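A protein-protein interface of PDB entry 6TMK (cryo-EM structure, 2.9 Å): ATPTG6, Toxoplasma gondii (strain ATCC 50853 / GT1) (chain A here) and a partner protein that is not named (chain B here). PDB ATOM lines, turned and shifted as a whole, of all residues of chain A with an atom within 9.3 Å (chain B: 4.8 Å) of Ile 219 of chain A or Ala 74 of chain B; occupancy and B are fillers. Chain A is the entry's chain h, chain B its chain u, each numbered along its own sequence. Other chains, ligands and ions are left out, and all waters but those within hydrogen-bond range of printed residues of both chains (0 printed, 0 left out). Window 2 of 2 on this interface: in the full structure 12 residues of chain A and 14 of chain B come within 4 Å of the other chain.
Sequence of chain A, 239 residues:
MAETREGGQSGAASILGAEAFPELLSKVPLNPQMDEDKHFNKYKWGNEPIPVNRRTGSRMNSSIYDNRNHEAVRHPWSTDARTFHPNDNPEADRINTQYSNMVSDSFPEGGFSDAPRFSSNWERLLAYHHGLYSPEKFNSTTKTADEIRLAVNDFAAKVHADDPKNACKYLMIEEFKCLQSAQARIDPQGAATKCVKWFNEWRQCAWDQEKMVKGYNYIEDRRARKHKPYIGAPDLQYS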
ATOM      1  N   TYR A 216      -9.640  -4.060 -32.983  1.00  0.00           N
ATOM      2  CA  TYR A 216     -10.523  -5.170 -33.300  1.00  0.00           C
ATOM      3  C   TYR A 216     -10.159  -6.317 -32.376  1.00  0.00           C
ATOM      4  O   TYR A 216      -9.001  -6.738 -32.329  1.00  0.00           O
ATOM      5  CB  TYR A 216     -10.398  -5.603 -34.760  1.00  0.00           C
ATOM      6  CG  TYR A 216     -10.937  -4.635 -35.779  1.00  0.00           C
ATOM      7  CD1 TYR A 216     -11.995  -3.800 -35.484  1.00  0.00           C
ATOM      8  CD2 TYR A 216     -10.400  -4.579 -37.049  1.00  0.00           C
ATOM      9  CE1 TYR A 216     -12.485  -2.924 -36.417  1.00  0.00           C
ATOM     10  CE2 TYR A 216     -10.884  -3.712 -37.985  1.00  0.00           C
ATOM     11  CZ  TYR A 216     -11.928  -2.888 -37.669  1.00  0.00           C
ATOM     12  OH  TYR A 216     -12.409  -2.020 -38.615  1.00  0.00           O
ATOM     13  N   ASN A 217     -11.148  -6.812 -31.647  1.00  0.00           N
ATOM     14  CA  ASN A 217     -10.952  -7.925 -30.742  1.00  0.00           C
ATOM     15  C   ASN A 217     -12.227  -8.746 -30.728  1.00  0.00           C
ATOM     16  O   ASN A 217     -13.220  -8.401 -31.371  1.00  0.00           O
ATOM     17  CB  ASN A 217     -10.579  -7.436 -29.345  1.00  0.00           C
ATOM     18  CG  ASN A 217      -9.767  -8.438 -28.579  1.00  0.00           C
ATOM     19  OD1 ASN A 217      -9.971  -9.642 -28.699  1.00  0.00           O
ATOM     20  ND2 ASN A 217      -8.840  -7.950 -27.782  1.00  0.00           N
ATOM     21  N   TYR A 218     -12.190  -9.842 -29.989  1.00  0.00           N
ATOM     22  CA  TYR A 218     -13.305 -10.765 -29.937  1.00  0.00           C
ATOM     23  C   TYR A 218     -13.475 -11.277 -28.520  1.00  0.00           C
ATOM     24  O   TYR A 218     -12.532 -11.288 -27.727  1.00  0.00           O
ATOM     25  CB  TYR A 218     -13.116 -11.937 -30.907  1.00  0.00           C
ATOM     26  CG  TYR A 218     -11.872 -12.746 -30.677  1.00  0.00           C
ATOM     27  CD1 TYR A 218     -11.918 -13.930 -29.974  1.00  0.00           C
ATOM     28  CD2 TYR A 218     -10.651 -12.330 -31.170  1.00  0.00           C
ATOM     29  CE1 TYR A 218     -10.791 -14.670 -29.764  1.00  0.00           C
ATOM     30  CE2 TYR A 218      -9.523 -13.062 -30.963  1.00  0.00           C
ATOM     31  CZ  TYR A 218      -9.592 -14.231 -30.257  1.00  0.00           C
ATOM     32  OH  TYR A 218      -8.452 -14.970 -30.054  1.00  0.00           O
ATOM     33  N   ILE A 219     -14.702 -11.682 -28.206  1.00  0.00           N
ATOM     34  CA  ILE A 219     -15.008 -12.246 -26.899  1.00  0.00           C
ATOM     35  C   ILE A 219     -14.399 -13.642 -26.853  1.00  0.00           C
ATOM     36  O   ILE A 219     -14.844 -14.546 -27.564  1.00  0.00           O
ATOM     37  CB  ILE A 219     -16.516 -12.286 -26.643  1.00  0.00           C
ATOM     38  CG1 ILE A 219     -17.076 -10.882 -26.495  1.00  0.00           C
ATOM     39  CG2 ILE A 219     -16.814 -13.038 -25.390  1.00  0.00           C
ATOM     40  CD1 ILE A 219     -18.500 -10.782 -26.898  1.00  0.00           C
ATOM     41  N   GLU A 220     -13.376 -13.820 -26.030  1.00  0.00           N
ATOM     42  CA  GLU A 220     -12.805 -15.136 -25.813  1.00  0.00           C
ATOM     43  C   GLU A 220     -13.674 -15.938 -24.858  1.00  0.00           C
ATOM     44  O   GLU A 220     -14.244 -15.396 -23.908  1.00  0.00           O
ATOM     45  CB  GLU A 220     -11.389 -15.019 -25.260  1.00  0.00           C
ATOM     46  CG  GLU A 220     -10.363 -14.634 -26.292  1.00  0.00           C
ATOM     47  CD  GLU A 220      -8.951 -14.715 -25.765  1.00  0.00           C
ATOM     48  OE1 GLU A 220      -8.719 -15.470 -24.798  1.00  0.00           O
ATOM     49  OE2 GLU A 220      -8.070 -14.021 -26.316  1.00  0.00           O
ATOM     50  N   ASP A 221     -13.770 -17.238 -25.115  1.00  0.00           N
ATOM     51  CA  ASP A 221     -14.568 -18.104 -24.272  1.00  0.00           C
ATOM     52  C   ASP A 221     -13.819 -18.450 -22.994  1.00  0.00           C
ATOM     53  O   ASP A 221     -12.603 -18.276 -22.881  1.00  0.00           O
ATOM     54  CB  ASP A 221     -14.944 -19.384 -25.009  1.00  0.00           C
ATOM     55  CG  ASP A 221     -16.092 -20.122 -24.346  1.00  0.00           C
ATOM     56  OD1 ASP A 221     -16.725 -19.546 -23.438  1.00  0.00           O
ATOM     57  OD2 ASP A 221     -16.357 -21.280 -24.726  1.00  0.00           O
ATOM     58  N   ARG A 222     -14.570 -18.945 -22.020  1.00  0.00           N
ATOM     59  CA  ARG A 222     -13.971 -19.383 -20.778  1.00  0.00           C
ATOM     60  C   ARG A 222     -12.981 -20.512 -21.035  1.00  0.00           C
ATOM     61  O   ARG A 222     -12.955 -21.137 -22.097  1.00  0.00           O
ATOM     62  CB  ARG A 222     -15.048 -19.842 -19.805  1.00  0.00           C
ATOM     63  CG  ARG A 222     -16.020 -18.767 -19.411  1.00  0.00           C
ATOM     64  CD  ARG A 222     -17.235 -19.358 -18.763  1.00  0.00           C
ATOM     65  NE  ARG A 222     -16.968 -19.803 -17.401  1.00  0.00           N
ATOM     66  CZ  ARG A 222     -17.594 -20.813 -16.811  1.00  0.00           C
ATOM     67  NH1 ARG A 222     -18.526 -21.495 -17.458  1.00  0.00           N
ATOM     68  NH2 ARG A 222     -17.279 -21.144 -15.570  1.00  0.00           N
ATOM     69  N   THR B  70     -21.795 -20.362 -23.348  1.00  0.00           N
ATOM     70  CA  THR B  70     -21.077 -19.176 -23.777  1.00  0.00           C
ATOM     71  C   THR B  70     -20.386 -19.388 -25.111  1.00  0.00           C
ATOM     72  O   THR B  70     -19.908 -18.415 -25.714  1.00  0.00           O
ATOM     73  CB  THR B  70     -20.026 -18.788 -22.728  1.00  0.00           C
ATOM     74  OG1 THR B  70     -19.088 -19.857 -22.573  1.00  0.00           O
ATOM     75  CG2 THR B  70     -20.676 -18.518 -21.405  1.00  0.00           C
ATOM     76  N   GLU B  71     -20.332 -20.633 -25.585  1.00  0.00           N
ATOM     77  CA  GLU B  71     -19.625 -20.945 -26.814  1.00  0.00           C
ATOM     78  C   GLU B  71     -20.268 -20.247 -27.997  1.00  0.00           C
ATOM     79  O   GLU B  71     -19.575 -19.807 -28.917  1.00  0.00           O
ATOM     80  CB  GLU B  71     -19.605 -22.458 -27.017  1.00  0.00           C
ATOM     81  CG  GLU B  71     -18.766 -23.192 -25.993  1.00  0.00           C
ATOM     82  CD  GLU B  71     -19.509 -23.445 -24.693  1.00  0.00           C
ATOM     83  OE1 GLU B  71     -18.930 -23.183 -23.618  1.00  0.00           O
ATOM     84  OE2 GLU B  71     -20.671 -23.900 -24.742  1.00  0.00           O
ATOM     85  N   SER B  72     -21.596 -20.136 -27.990  1.00  0.00           N
ATOM     86  CA  SER B  72     -22.289 -19.487 -29.095  1.00  0.00           C
ATOM     87  C   SER B  72     -21.869 -18.031 -29.215  1.00  0.00           C
ATOM     88  O   SER B  72     -21.561 -17.547 -30.308  1.00  0.00           O
ATOM     89  CB  SER B  72     -23.796 -19.602 -28.898  1.00  0.00           C
ATOM     90  OG  SER B  72     -24.182 -20.956 -28.766  1.00  0.00           O
ATOM     91  N   VAL B  73     -21.848 -17.317 -28.090  1.00  0.00           N
ATOM     92  CA  VAL B  73     -21.475 -15.906 -28.096  1.00  0.00           C
ATOM     93  C   VAL B  73     -20.023 -15.747 -28.513  1.00  0.00           C
ATOM     94  O   VAL B  73     -19.680 -14.889 -29.339  1.00  0.00           O
ATOM     95  CB  VAL B  73     -21.731 -15.289 -26.711  1.00  0.00           C
ATOM     96  CG1 VAL B  73     -21.057 -13.943 -26.582  1.00  0.00           C
ATOM     97  CG2 VAL B  73     -23.201 -15.165 -26.472  1.00  0.00           C
ATOM     98  N   ALA B  74     -19.143 -16.565 -27.935  1.00  0.00           N
ATOM     99  CA  ALA B  74     -17.730 -16.463 -28.274  1.00  0.00           C
ATOM    100  C   ALA B  74     -17.506 -16.725 -29.757  1.00  0.00           C
ATOM    101  O   ALA B  74     -16.738 -16.015 -30.418  1.00  0.00           O
ATOM    102  CB  ALA B  74     -16.930 -17.435 -27.421  1.00  0.00           C
ATOM    103  N   LEU B  75     -18.187 -17.732 -30.299  1.00  0.00           N
ATOM    104  CA  LEU B  75     -18.029 -18.082 -31.699  1.00  0.00           C
ATOM    105  C   LEU B  75     -18.600 -17.002 -32.604  1.00  0.00           C
ATOM    106  O   LEU B  75     -18.046 -16.724 -33.669  1.00  0.00           O
ATOM    107  CB  LEU B  75     -18.695 -19.425 -31.960  1.00  0.00           C
ATOM    108  CG  LEU B  75     -18.548 -20.020 -33.351  1.00  0.00           C
ATOM    109  CD1 LEU B  75     -17.119 -20.426 -33.616  1.00  0.00           C
ATOM    110  CD2 LEU B  75     -19.475 -21.194 -33.478  1.00  0.00           C
ATOM    111  N   GLN B  76     -19.721 -16.401 -32.211  1.00  0.00           N
ATOM    112  CA  GLN B  76     -20.290 -15.308 -32.986  1.00  0.00           C
ATOM    113  C   GLN B  76     -19.319 -14.138 -33.061  1.00  0.00           C
ATOM    114  O   GLN B  76     -19.103 -13.553 -34.131  1.00  0.00           O
ATOM    115  CB  GLN B  76     -21.614 -14.882 -32.361  1.00  0.00           C
ATOM    116  CG  GLN B  76     -22.763 -15.801 -32.679  1.00  0.00           C
ATOM    117  CD  GLN B  76     -24.024 -15.431 -31.933  1.00  0.00           C
ATOM    118  OE1 GLN B  76     -24.139 -14.333 -31.394  1.00  0.00           O
ATOM    119  NE2 GLN B  76     -24.973 -16.354 -31.884  1.00  0.00           N
ATOM    120  N   SER B  77     -18.730 -13.778 -31.921  1.00  0.00           N
ATOM    121  CA  SER B  77     -17.731 -12.720 -31.902  1.00  0.00           C
ATOM    122  C   SER B  77     -16.567 -13.060 -32.822  1.00  0.00           C
ATOM    123  O   SER B  77     -16.117 -12.227 -33.623  1.00  0.00           O
ATOM    124  CB  SER B  77     -17.252 -12.499 -30.469  1.00  0.00           C
ATOM    125  OG  SER B  77     -16.612 -11.252 -30.311  1.00  0.00           O
ATOM    126  N   ARG B  78     -16.068 -14.291 -32.719  1.00  0.00           N
ATOM    127  CA  ARG B  78     -14.940 -14.703 -33.536  1.00  0.00           C
ATOM    128  C   ARG B  78     -15.285 -14.707 -35.020  1.00  0.00           C
ATOM    129  O   ARG B  78     -14.433 -14.394 -35.857  1.00  0.00           O
ATOM    130  CB  ARG B  78     -14.475 -16.077 -33.067  1.00  0.00           C
ATOM    131  CG  ARG B  78     -13.191 -16.561 -33.657  1.00  0.00           C
ATOM    132  CD  ARG B  78     -12.052 -15.639 -33.397  1.00  0.00           C
ATOM    133  NE  ARG B  78     -10.814 -16.175 -33.931  1.00  0.00           N
ATOM    134  CZ  ARG B  78      -9.730 -15.452 -34.149  1.00  0.00           C
ATOM    135  NH1 ARG B  78      -9.718 -14.169 -33.873  1.00  0.00           N
ATOM    136  NH2 ARG B  78      -8.657 -16.015 -34.645  1.00  0.00           N
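N of Ile 219 of chain A is in hydrogen-bond range of OG of Ser 77 of chain B (2.9 Å). The side-chain carboxylate (OE1) of Glu 71 of chain B sits close to the side-chain carboxylate (OD2) of Asp 221 of chain A (3.4 Å). OD1 of Asp 221 of chain A is in hydrogen-bond range of OG1 of Thr 70 of chain B (2.5 Å).
OG1 of Thr 70 of chain B sits at hydrogen-bond distance from OE1 of Glu 71 of chain B (3.5 Å).
Among the printed residues, merely in contact across the chains: Tyr 218 of chain A with Arg 78 of chain B (3.1 Å), Tyr 218 of chain A with Ser 77 of chain B (3.4 Å), Ile 219 of chain A with Ala 74 of chain B (3.5 Å) and Asp 221 of chain A with Ala 74 of chain B (3.7 Å).
Printed residues of chain B within 4 Å of Tyr 218 of chain A: Ser 77 and Arg 78. Ile 219 of chain A touches just these residues of chain B: Ala 74 and Ser 77. Of the printed residues of chain B, Asp 221 of chain A touches Thr 70 (2.5 Å), Glu 71 (3.3 Å) and Ala 74 (3.7 Å). Of the printed residues of chain A, Thr 70 of chain B touches Asp 221 (2.5 Å). Of the printed residues of chain A, Glu 71 of chain B touches Asp 221. Ala 74 of chain B touches just these residues of chain A: Ile 219 and Asp 221. Ser 77 of chain B touches just these residues of chain A: Tyr 218 (3.4 Å) and Ile 219 (2.9 Å). Printed residues of chain A within 4 Å of Arg 78 of chain B: Tyr 218 (3.1 Å). The nearest residue of chain B that does not touch Ile 219 of chain A is Val 73 of chain B (4.1 Å). The nearest printed residue of chain A that does not touch Thr 70 of chain B is Arg 222 of chain A (4.3 Å).
Of the 9 printed residues of chain B, 5 touch a printed residue of chain A. Printed residues of chain B that touch a printed residue of chain A: Thr 70, Glu 71, Ala 74, Ser 77 and Arg 78. Hydrophobic or aromatic side chains of chain B within 4 Å of the printed part of chain A: Ala 74. Along chain B the printed residues that touch a printed residue of chain A span positions 70 to 78. Of the 7 printed residues of chain A, 3 touch a printed residue of chain B. Hydrophobic or aromatic side chains of chain A within 4 Å of the printed part of chain B: Tyr 218 and Ile 219. Along chain A the printed residues that touch a printed residue of chain B span positions 218 to 221. Among the printed residues, 7 pairs touch across the chains.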
